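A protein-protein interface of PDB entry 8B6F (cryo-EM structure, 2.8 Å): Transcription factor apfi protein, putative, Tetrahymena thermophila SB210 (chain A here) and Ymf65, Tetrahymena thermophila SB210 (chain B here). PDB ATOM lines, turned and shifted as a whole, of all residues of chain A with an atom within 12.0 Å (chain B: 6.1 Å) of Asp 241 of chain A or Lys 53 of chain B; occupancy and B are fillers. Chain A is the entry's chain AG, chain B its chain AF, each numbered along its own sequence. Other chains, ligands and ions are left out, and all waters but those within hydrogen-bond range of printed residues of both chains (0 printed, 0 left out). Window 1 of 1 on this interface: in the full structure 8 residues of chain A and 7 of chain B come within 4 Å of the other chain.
N of Ser 244 of chain A sits close to OD1 of Asp 241 of chain A, at 3.3 Å.
NZ of Lys 169 of chain B is in hydrogen-bond range of O of Ser 171 of chain B (3.1 Å).
The side-chain amide oxygen (OD1) of Asn 121 of chain B sits close to the backbone carbonyl oxygen (O) of Tyr 123 of chain B (2.8 Å).
Glu 239 of chain A touches Lys 53 of chain B (O to CG, 3.99 Å).
Asn 121 of chain B touches Glu 239 of chain A (ND2 to OE1, 3.7 Å).
Lys 53 of chain B touches Asp 241 of chain A.
OG of Ser 171 of chain B touches CD2 of His 242 of chain A, 3.2 Å away.
His 242 of chain A touches Lys 173 of chain B (NE2 to N, 3.9 Å).
Ser 244 of chain A touches Ile 51 of chain B (O to CG2, 3.9 Å).
Leu 247 of chain A touches Ile 51 of chain B.
Gln 248 of chain A touches Ile 51 of chain B.
Arg 251 of chain A touches Ile 51 of chain B.
Of the printed residues of chain B, Asp 241 of chain A touches Lys 53.
Of the printed residues of chain A, Lys 53 of chain B touches Glu 239 and Asp 241.
No residue of chain A comes within 4 Å of Ile 52 of chain B.
No residue of chain A comes within 4 Å of Gln 54 of chain B.
No residue of chain A comes within 4 Å of Asn 55 of chain B.
No residue of chain A comes within 4 Å of Ser 124 of chain B.
Of the printed residues of chain B, Glu 239 of chain A touches Lys 53 (3.99 Å) and Asn 121 (3.7 Å).
Printed residues of chain B within 4 Å of Ser 244 of chain A: Ile 51 (3.9 Å).
Of the printed residues of chain B, Leu 247 of chain A touches Ile 51.
Printed residues of chain A within 4 Å of Lys 173 of chain B: His 242.
Ala 238 of chain A touches none of the printed residues of chain B.
Ala 246 of chain A touches none of the printed residues of chain B.
The nearest printed residue of chain B that does not touch Asp 241 of chain A is Lys 169 of chain B (4.02 Å).
The nearest printed residue of chain A that does not touch Lys 53 of chain B is Ser 244 of chain A (4.03 Å).
Of the 12 printed residues of chain B, 5 touch a printed residue of chain A.
Hydrophobic or aromatic side chains of chain B within 4 Å of the printed part of chain A: Ile 51.
Hydrophobic or aromatic side chains of chain A within 4 Å of the printed part of chain B: His 242 and Leu 247.
Among the printed residues, no Asp or Glu carboxylate lies within 4 Å of a Lys or Arg side-chain nitrogen of the other chain.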
ATOM      1  N   ASP A 232       6.846   7.728 -13.585  1.00  0.00           N
ATOM      2  CA  ASP A 232       6.020   8.776 -14.176  1.00  0.00           C
ATOM      3  C   ASP A 232       6.849   9.700 -15.058  1.00  0.00           C
ATOM      4  O   ASP A 232       6.407  10.103 -16.139  1.00  0.00           O
ATOM      5  CB  ASP A 232       5.321   9.576 -13.078  1.00  0.00           C
ATOM      6  CG  ASP A 232       4.321   8.748 -12.304  1.00  0.00           C
ATOM      7  OD1 ASP A 232       4.194   7.543 -12.596  1.00  0.00           O
ATOM      8  OD2 ASP A 232       3.656   9.303 -11.406  1.00  0.00           O
ATOM      9  N   ARG A 233       8.056  10.052 -14.609  1.00  0.00           N
ATOM     10  CA  ARG A 233       8.911  10.934 -15.397  1.00  0.00           C
ATOM     11  C   ARG A 233       9.327  10.279 -16.708  1.00  0.00           C
ATOM     12  O   ARG A 233       9.343  10.935 -17.756  1.00  0.00           O
ATOM     13  CB  ARG A 233      10.144  11.332 -14.587  1.00  0.00           C
ATOM     14  CG  ARG A 233      10.946  12.462 -15.218  1.00  0.00           C
ATOM     15  CD  ARG A 233      12.347  12.558 -14.644  1.00  0.00           C
ATOM     16  NE  ARG A 233      13.147  11.381 -14.973  1.00  0.00           N
ATOM     17  CZ  ARG A 233      13.427  10.391 -14.136  1.00  0.00           C
ATOM     18  NH1 ARG A 233      13.012  10.402 -12.880  1.00  0.00           N
ATOM     19  NH2 ARG A 233      14.147   9.361 -14.572  1.00  0.00           N
ATOM     20  N   ILE A 234       9.660   8.989 -16.676  1.00  0.00           N
ATOM     21  CA  ILE A 234      10.032   8.296 -17.906  1.00  0.00           C
ATOM     22  C   ILE A 234       8.854   8.257 -18.871  1.00  0.00           C
ATOM     23  O   ILE A 234       9.013   8.479 -20.077  1.00  0.00           O
ATOM     24  CB  ILE A 234      10.549   6.882 -17.583  1.00  0.00           C
ATOM     25  CG1 ILE A 234      11.828   6.963 -16.748  1.00  0.00           C
ATOM     26  CG2 ILE A 234      10.804   6.095 -18.865  1.00  0.00           C
ATOM     27  CD1 ILE A 234      12.270   5.637 -16.164  1.00  0.00           C
ATOM     28  N   THR A 235       7.660   7.955 -18.363  1.00  0.00           N
ATOM     29  CA  THR A 235       6.480   7.932 -19.220  1.00  0.00           C
ATOM     30  C   THR A 235       6.220   9.302 -19.832  1.00  0.00           C
ATOM     31  O   THR A 235       5.887   9.410 -21.017  1.00  0.00           O
ATOM     32  CB  THR A 235       5.275   7.439 -18.426  1.00  0.00           C
ATOM     33  OG1 THR A 235       5.546   6.110 -17.962  1.00  0.00           O
ATOM     34  CG2 THR A 235       4.012   7.436 -19.280  1.00  0.00           C
ATOM     35  N   ALA A 236       6.360  10.364 -19.036  1.00  0.00           N
ATOM     36  CA  ALA A 236       6.150  11.708 -19.560  1.00  0.00           C
ATOM     37  C   ALA A 236       7.191  12.049 -20.616  1.00  0.00           C
ATOM     38  O   ALA A 236       6.859  12.604 -21.668  1.00  0.00           O
ATOM     39  CB  ALA A 236       6.186  12.727 -18.422  1.00  0.00           C
ATOM     40  N   GLU A 237       8.458  11.715 -20.359  1.00  0.00           N
ATOM     41  CA  GLU A 237       9.505  11.986 -21.338  1.00  0.00           C
ATOM     42  C   GLU A 237       9.275  11.217 -22.629  1.00  0.00           C
ATOM     43  O   GLU A 237       9.691  11.667 -23.701  1.00  0.00           O
ATOM     44  CB  GLU A 237      10.874  11.634 -20.756  1.00  0.00           C
ATOM     45  CG  GLU A 237      11.337  12.574 -19.662  1.00  0.00           C
ATOM     46  CD  GLU A 237      12.664  12.157 -19.068  1.00  0.00           C
ATOM     47  OE1 GLU A 237      13.254  11.176 -19.566  1.00  0.00           O
ATOM     48  OE2 GLU A 237      13.118  12.807 -18.104  1.00  0.00           O
ATOM     49  N   ALA A 238       8.625  10.057 -22.551  1.00  0.00           N
ATOM     50  CA  ALA A 238       8.298   9.312 -23.758  1.00  0.00           C
ATOM     51  C   ALA A 238       7.416  10.114 -24.705  1.00  0.00           C
ATOM     52  O   ALA A 238       7.378   9.811 -25.903  1.00  0.00           O
ATOM     53  CB  ALA A 238       7.606   7.997 -23.396  1.00  0.00           C
ATOM     54  N   GLU A 239       6.709  11.128 -24.202  1.00  0.00           N
ATOM     55  CA  GLU A 239       5.811  11.928 -25.022  1.00  0.00           C
ATOM     56  C   GLU A 239       6.153  13.411 -25.040  1.00  0.00           C
ATOM     57  O   GLU A 239       5.501  14.167 -25.769  1.00  0.00           O
ATOM     58  CB  GLU A 239       4.360  11.748 -24.549  1.00  0.00           C
ATOM     59  CG  GLU A 239       4.113  12.184 -23.112  1.00  0.00           C
ATOM     60  CD  GLU A 239       2.677  11.957 -22.679  1.00  0.00           C
ATOM     61  OE1 GLU A 239       1.901  11.383 -23.471  1.00  0.00           O
ATOM     62  OE2 GLU A 239       2.324  12.353 -21.549  1.00  0.00           O
ATOM     63  N   TYR A 240       7.134  13.858 -24.260  1.00  0.00           N
ATOM     64  CA  TYR A 240       7.543  15.253 -24.316  1.00  0.00           C
ATOM     65  C   TYR A 240       8.138  15.572 -25.682  1.00  0.00           C
ATOM     66  O   TYR A 240       8.772  14.730 -26.322  1.00  0.00           O
ATOM     67  CB  TYR A 240       8.567  15.565 -23.219  1.00  0.00           C
ATOM     68  CG  TYR A 240       7.978  15.809 -21.842  1.00  0.00           C
ATOM     69  CD1 TYR A 240       6.756  16.453 -21.681  1.00  0.00           C
ATOM     70  CD2 TYR A 240       8.656  15.401 -20.701  1.00  0.00           C
ATOM     71  CE1 TYR A 240       6.224  16.675 -20.427  1.00  0.00           C
ATOM     72  CE2 TYR A 240       8.131  15.618 -19.443  1.00  0.00           C
ATOM     73  CZ  TYR A 240       6.917  16.256 -19.312  1.00  0.00           C
ATOM     74  OH  TYR A 240       6.394  16.474 -18.059  1.00  0.00           O
ATOM     75  N   ASP A 241       7.928  16.805 -26.127  1.00  0.00           N
ATOM     76  CA  ASP A 241       8.387  17.280 -27.424  1.00  0.00           C
ATOM     77  C   ASP A 241       9.555  18.246 -27.239  1.00  0.00           C
ATOM     78  O   ASP A 241       9.975  18.549 -26.122  1.00  0.00           O
ATOM     79  CB  ASP A 241       7.239  17.939 -28.190  1.00  0.00           C
ATOM     80  CG  ASP A 241       6.557  19.030 -27.392  1.00  0.00           C
ATOM     81  OD1 ASP A 241       6.534  18.930 -26.148  1.00  0.00           O
ATOM     82  OD2 ASP A 241       6.048  19.989 -28.008  1.00  0.00           O
ATOM     83  N   HIS A 242      10.083  18.731 -28.365  1.00  0.00           N
ATOM     84  CA  HIS A 242      11.227  19.636 -28.317  1.00  0.00           C
ATOM     85  C   HIS A 242      10.889  20.911 -27.559  1.00  0.00           C
ATOM     86  O   HIS A 242      11.707  21.415 -26.782  1.00  0.00           O
ATOM     87  CB  HIS A 242      11.696  19.966 -29.734  1.00  0.00           C
ATOM     88  CG  HIS A 242      12.270  18.796 -30.468  1.00  0.00           C
ATOM     89  ND1 HIS A 242      13.570  18.372 -30.293  1.00  0.00           N
ATOM     90  CD2 HIS A 242      11.722  17.957 -31.377  1.00  0.00           C
ATOM     91  CE1 HIS A 242      13.798  17.325 -31.063  1.00  0.00           C
ATOM     92  NE2 HIS A 242      12.693  17.052 -31.732  1.00  0.00           N
ATOM     93  N   GLU A 243       9.691  21.454 -27.778  1.00  0.00           N
ATOM     94  CA  GLU A 243       9.295  22.665 -27.068  1.00  0.00           C
ATOM     95  C   GLU A 243       9.220  22.423 -25.566  1.00  0.00           C
ATOM     96  O   GLU A 243       9.649  23.269 -24.773  1.00  0.00           O
ATOM     97  CB  GLU A 243       7.955  23.169 -27.600  1.00  0.00           C
ATOM     98  CG  GLU A 243       7.620  24.574 -27.146  1.00  0.00           C
ATOM     99  CD  GLU A 243       6.376  25.119 -27.813  1.00  0.00           C
ATOM    100  OE1 GLU A 243       5.751  24.377 -28.597  1.00  0.00           O
ATOM    101  OE2 GLU A 243       6.026  26.289 -27.555  1.00  0.00           O
ATOM    102  N   SER A 244       8.679  21.277 -25.154  1.00  0.00           N
ATOM    103  CA  SER A 244       8.604  20.972 -23.729  1.00  0.00           C
ATOM    104  C   SER A 244       9.992  20.835 -23.121  1.00  0.00           C
ATOM    105  O   SER A 244      10.247  21.333 -22.020  1.00  0.00           O
ATOM    106  CB  SER A 244       7.799  19.692 -23.505  1.00  0.00           C
ATOM    107  OG  SER A 244       6.461  19.844 -23.947  1.00  0.00           O
ATOM    108  N   LEU A 245      10.905  20.158 -23.821  1.00  0.00           N
ATOM    109  CA  LEU A 245      12.267  20.023 -23.317  1.00  0.00           C
ATOM    110  C   LEU A 245      12.953  21.379 -23.216  1.00  0.00           C
ATOM    111  O   LEU A 245      13.637  21.664 -22.228  1.00  0.00           O
ATOM    112  CB  LEU A 245      13.071  19.082 -24.212  1.00  0.00           C
ATOM    113  CG  LEU A 245      12.529  17.658 -24.336  1.00  0.00           C
ATOM    114  CD1 LEU A 245      13.307  16.889 -25.385  1.00  0.00           C
ATOM    115  CD2 LEU A 245      12.583  16.941 -22.998  1.00  0.00           C
ATOM    116  N   ALA A 246      12.775  22.231 -24.226  1.00  0.00           N
ATOM    117  CA  ALA A 246      13.356  23.569 -24.172  1.00  0.00           C
ATOM    118  C   ALA A 246      12.801  24.359 -22.996  1.00  0.00           C
ATOM    119  O   ALA A 246      13.545  25.066 -22.307  1.00  0.00           O
ATOM    120  CB  ALA A 246      13.091  24.307 -25.484  1.00  0.00           C
ATOM    121  N   LEU A 247      11.498  24.241 -22.742  1.00  0.00           N
ATOM    122  CA  LEU A 247      10.901  24.919 -21.596  1.00  0.00           C
ATOM    123  C   LEU A 247      11.476  24.399 -20.287  1.00  0.00           C
ATOM    124  O   LEU A 247      11.719  25.176 -19.357  1.00  0.00           O
ATOM    125  CB  LEU A 247       9.383  24.750 -21.617  1.00  0.00           C
ATOM    126  CG  LEU A 247       8.620  25.501 -22.707  1.00  0.00           C
ATOM    127  CD1 LEU A 247       7.165  25.070 -22.734  1.00  0.00           C
ATOM    128  CD2 LEU A 247       8.726  26.999 -22.481  1.00  0.00           C
ATOM    129  N   GLN A 248      11.701  23.088 -20.190  1.00  0.00           N
ATOM    130  CA  GLN A 248      12.314  22.541 -18.984  1.00  0.00           C
ATOM    131  C   GLN A 248      13.685  23.158 -18.749  1.00  0.00           C
ATOM    132  O   GLN A 248      14.007  23.582 -17.633  1.00  0.00           O
ATOM    133  CB  GLN A 248      12.422  21.021 -19.091  1.00  0.00           C
ATOM    134  CG  GLN A 248      11.089  20.304 -19.010  1.00  0.00           C
ATOM    135  CD  GLN A 248      11.228  18.808 -19.167  1.00  0.00           C
ATOM    136  OE1 GLN A 248      12.335  18.280 -19.239  1.00  0.00           O
ATOM    137  NE2 GLN A 248      10.100  18.114 -19.223  1.00  0.00           N
ATOM    138  N   LYS A 249      14.516  23.205 -19.788  1.00  0.00           N
ATOM    139  CA  LYS A 249      15.843  23.793 -19.639  1.00  0.00           C
ATOM    140  C   LYS A 249      15.746  25.274 -19.293  1.00  0.00           C
ATOM    141  O   LYS A 249      16.517  25.778 -18.470  1.00  0.00           O
ATOM    142  CB  LYS A 249      16.659  23.584 -20.915  1.00  0.00           C
ATOM    143  CG  LYS A 249      17.373  22.238 -20.979  1.00  0.00           C
ATOM    144  CD  LYS A 249      16.385  21.082 -21.031  1.00  0.00           C
ATOM    145  CE  LYS A 249      17.089  19.737 -21.032  1.00  0.00           C
ATOM    146  NZ  LYS A 249      16.121  18.604 -20.984  1.00  0.00           N
ATOM    147  N   MET A 250      14.796  25.986 -19.904  1.00  0.00           N
ATOM    148  CA  MET A 250      14.645  27.412 -19.627  1.00  0.00           C
ATOM    149  C   MET A 250      14.238  27.665 -18.182  1.00  0.00           C
ATOM    150  O   MET A 250      14.766  28.576 -17.535  1.00  0.00           O
ATOM    151  CB  MET A 250      13.618  28.023 -20.578  1.00  0.00           C
ATOM    152  CG  MET A 250      14.101  28.152 -22.008  1.00  0.00           C
ATOM    153  SD  MET A 250      12.815  28.762 -23.107  1.00  0.00           S
ATOM    154  CE  MET A 250      13.639  28.597 -24.683  1.00  0.00           C
ATOM    155  N   ARG A 251      13.301  26.878 -17.653  1.00  0.00           N
ATOM    156  CA  ARG A 251      12.898  27.073 -16.263  1.00  0.00           C
ATOM    157  C   ARG A 251      14.031  26.713 -15.311  1.00  0.00           C
ATOM    158  O   ARG A 251      14.192  27.349 -14.263  1.00  0.00           O
ATOM    159  CB  ARG A 251      11.641  26.260 -15.950  1.00  0.00           C
ATOM    160  CG  ARG A 251      11.840  24.754 -15.940  1.00  0.00           C
ATOM    161  CD  ARG A 251      10.640  24.037 -15.349  1.00  0.00           C
ATOM    162  NE  ARG A 251      10.841  22.594 -15.315  1.00  0.00           N
ATOM    163  CZ  ARG A 251      11.529  21.951 -14.382  1.00  0.00           C
ATOM    164  NH1 ARG A 251      12.104  22.594 -13.380  1.00  0.00           N
ATOM    165  NH2 ARG A 251      11.645  20.629 -14.460  1.00  0.00           N
ATOM    166  N   ILE B  51       5.459  22.744 -16.935  1.00  0.00           N
ATOM    167  CA  ILE B  51       5.616  22.017 -18.191  1.00  0.00           C
ATOM    168  C   ILE B  51       4.505  20.980 -18.292  1.00  0.00           C
ATOM    169  O   ILE B  51       4.407  20.080 -17.452  1.00  0.00           O
ATOM    170  CB  ILE B  51       6.998  21.353 -18.271  1.00  0.00           C
ATOM    171  CG1 ILE B  51       8.103  22.358 -17.926  1.00  0.00           C
ATOM    172  CG2 ILE B  51       7.226  20.763 -19.653  1.00  0.00           C
ATOM    173  CD1 ILE B  51       8.047  23.638 -18.722  1.00  0.00           C
ATOM    174  N   ILE B  52       3.672  21.098 -19.323  1.00  0.00           N
ATOM    175  CA  ILE B  52       2.519  20.222 -19.497  1.00  0.00           C
ATOM    176  C   ILE B  52       2.422  19.806 -20.957  1.00  0.00           C
ATOM    177  O   ILE B  52       2.703  20.599 -21.862  1.00  0.00           O
ATOM    178  CB  ILE B  52       1.213  20.900 -19.035  1.00  0.00           C
ATOM    179  CG1 ILE B  52       0.967  22.191 -19.821  1.00  0.00           C
ATOM    180  CG2 ILE B  52       1.274  21.190 -17.542  1.00  0.00           C
ATOM    181  CD1 ILE B  52      -0.400  22.798 -19.585  1.00  0.00           C
ATOM    182  N   LYS B  53       2.022  18.554 -21.184  1.00  0.00           N
ATOM    183  CA  LYS B  53       1.754  18.027 -22.525  1.00  0.00           C
ATOM    184  C   LYS B  53       0.482  17.188 -22.416  1.00  0.00           C
ATOM    185  O   LYS B  53       0.539  15.990 -22.129  1.00  0.00           O
ATOM    186  CB  LYS B  53       2.929  17.211 -23.051  1.00  0.00           C
ATOM    187  CG  LYS B  53       2.864  16.905 -24.542  1.00  0.00           C
ATOM    188  CD  LYS B  53       3.087  18.158 -25.378  1.00  0.00           C
ATOM    189  CE  LYS B  53       3.178  17.836 -26.861  1.00  0.00           C
ATOM    190  NZ  LYS B  53       1.934  17.207 -27.377  1.00  0.00           N
ATOM    191  N   GLN B  54      -0.663  17.824 -22.649  1.00  0.00           N
ATOM    192  CA  GLN B  54      -1.940  17.153 -22.452  1.00  0.00           C
ATOM    193  C   GLN B  54      -2.207  16.166 -23.579  1.00  0.00           C
ATOM    194  O   GLN B  54      -2.076  16.500 -24.761  1.00  0.00           O
ATOM    195  CB  GLN B  54      -3.075  18.173 -22.375  1.00  0.00           C
ATOM    196  CG  GLN B  54      -3.040  19.043 -21.134  1.00  0.00           C
ATOM    197  CD  GLN B  54      -4.320  19.834 -20.936  1.00  0.00           C
ATOM    198  OE1 GLN B  54      -4.700  20.141 -19.806  1.00  0.00           O
ATOM    199  NE2 GLN B  54      -4.988  20.178 -22.033  1.00  0.00           N
ATOM    200  N   ASN B  55      -2.588  14.950 -23.206  1.00  0.00           N
ATOM    201  CA  ASN B  55      -2.989  13.962 -24.191  1.00  0.00           C
ATOM    202  C   ASN B  55      -4.363  14.327 -24.752  1.00  0.00           C
ATOM    203  O   ASN B  55      -5.257  14.721 -23.996  1.00  0.00           O
ATOM    204  CB  ASN B  55      -3.023  12.573 -23.556  1.00  0.00           C
ATOM    205  CG  ASN B  55      -3.317  11.480 -24.558  1.00  0.00           C
ATOM    206  OD1 ASN B  55      -4.326  11.519 -25.260  1.00  0.00           O
ATOM    207  ND2 ASN B  55      -2.433  10.494 -24.632  1.00  0.00           N
ATOM    208  N   ASN B 121       1.458   9.065 -28.156  1.00  0.00           N
ATOM    209  CA  ASN B 121       0.989  10.424 -28.413  1.00  0.00           C
ATOM    210  C   ASN B 121       2.031  11.169 -29.239  1.00  0.00           C
ATOM    211  O   ASN B 121       3.045  11.627 -28.705  1.00  0.00           O
ATOM    212  CB  ASN B 121       0.703  11.147 -27.100  1.00  0.00           C
ATOM    213  CG  ASN B 121       0.286  12.588 -27.306  1.00  0.00           C
ATOM    214  OD1 ASN B 121      -0.137  12.974 -28.395  1.00  0.00           O
ATOM    215  ND2 ASN B 121       0.402  13.392 -26.257  1.00  0.00           N
ATOM    216  N   TYR B 123       0.516  13.463 -31.571  1.00  0.00           N
ATOM    217  CA  TYR B 123      -0.454  14.349 -32.200  1.00  0.00           C
ATOM    218  C   TYR B 123      -0.956  15.347 -31.169  1.00  0.00           C
ATOM    219  O   TYR B 123      -1.277  14.968 -30.038  1.00  0.00           O
ATOM    220  CB  TYR B 123      -1.616  13.542 -32.785  1.00  0.00           C
ATOM    221  CG  TYR B 123      -1.155  12.370 -33.620  1.00  0.00           C
ATOM    222  CD1 TYR B 123      -0.855  11.147 -33.031  1.00  0.00           C
ATOM    223  CD2 TYR B 123      -1.000  12.490 -34.994  1.00  0.00           C
ATOM    224  CE1 TYR B 123      -0.425  10.076 -33.787  1.00  0.00           C
ATOM    225  CE2 TYR B 123      -0.569  11.425 -35.760  1.00  0.00           C
ATOM    226  CZ  TYR B 123      -0.284  10.221 -35.150  1.00  0.00           C
ATOM    227  OH  TYR B 123       0.145   9.158 -35.910  1.00  0.00           O
ATOM    228  N   SER B 124      -1.027  16.616 -31.561  1.00  0.00           N
ATOM    229  CA  SER B 124      -1.407  17.681 -30.646  1.00  0.00           C
ATOM    230  C   SER B 124      -2.927  17.805 -30.560  1.00  0.00           C
ATOM    231  O   SER B 124      -3.679  17.136 -31.272  1.00  0.00           O
ATOM    232  CB  SER B 124      -0.786  19.006 -31.087  1.00  0.00           C
ATOM    233  OG  SER B 124      -1.222  19.373 -32.384  1.00  0.00           O
ATOM    234  N   ILE B 125      -3.378  18.681 -29.660  1.00  0.00           N
ATOM    235  CA  ILE B 125      -4.811  18.904 -29.498  1.00  0.00           C
ATOM    236  C   ILE B 125      -5.386  19.620 -30.710  1.00  0.00           C
ATOM    237  O   ILE B 125      -6.546  19.399 -31.078  1.00  0.00           O
ATOM    238  CB  ILE B 125      -5.080  19.675 -28.191  1.00  0.00           C
ATOM    239  CG1 ILE B 125      -4.825  18.759 -26.991  1.00  0.00           C
ATOM    240  CG2 ILE B 125      -6.502  20.233 -28.166  1.00  0.00           C
ATOM    241  CD1 ILE B 125      -4.886  19.456 -25.653  1.00  0.00           C
ATOM    242  N   LYS B 169       2.720  17.031 -36.929  1.00  0.00           N
ATOM    243  CA  LYS B 169       3.960  17.087 -36.170  1.00  0.00           C
ATOM    244  C   LYS B 169       5.152  17.013 -37.115  1.00  0.00           C
ATOM    245  O   LYS B 169       5.152  16.242 -38.078  1.00  0.00           O
ATOM    246  CB  LYS B 169       4.008  15.942 -35.160  1.00  0.00           C
ATOM    247  CG  LYS B 169       5.240  15.932 -34.274  1.00  0.00           C
ATOM    248  CD  LYS B 169       5.162  14.800 -33.268  1.00  0.00           C
ATOM    249  CE  LYS B 169       6.417  14.711 -32.424  1.00  0.00           C
ATOM    250  NZ  LYS B 169       6.635  15.945 -31.624  1.00  0.00           N
ATOM    251  N   SER B 171       9.017  17.688 -35.981  1.00  0.00           N
ATOM    252  CA  SER B 171      10.267  17.214 -35.406  1.00  0.00           C
ATOM    253  C   SER B 171       9.985  16.227 -34.282  1.00  0.00           C
ATOM    254  O   SER B 171       9.169  16.505 -33.396  1.00  0.00           O
ATOM    255  CB  SER B 171      11.097  18.383 -34.880  1.00  0.00           C
ATOM    256  OG  SER B 171      10.346  19.151 -33.955  1.00  0.00           O
ATOM    257  N   LYS B 173      11.562  13.358 -31.273  1.00  0.00           N
ATOM    258  CA  LYS B 173      12.661  13.079 -30.353  1.00  0.00           C
ATOM    259  C   LYS B 173      13.065  11.620 -30.546  1.00  0.00           C
ATOM    260  O   LYS B 173      12.684  10.730 -29.788  1.00  0.00           O
ATOM    261  CB  LYS B 173      12.247  13.374 -28.915  1.00  0.00           C
ATOM    262  CG  LYS B 173      13.327  13.092 -27.878  1.00  0.00           C
ATOM    263  CD  LYS B 173      14.557  13.961 -28.097  1.00  0.00           C
ATOM    264  CE  LYS B 173      15.587  13.750 -26.998  1.00  0.00           C
ATOM    265  NZ  LYS B 173      16.056  12.338 -26.928  1.00  0.00           N
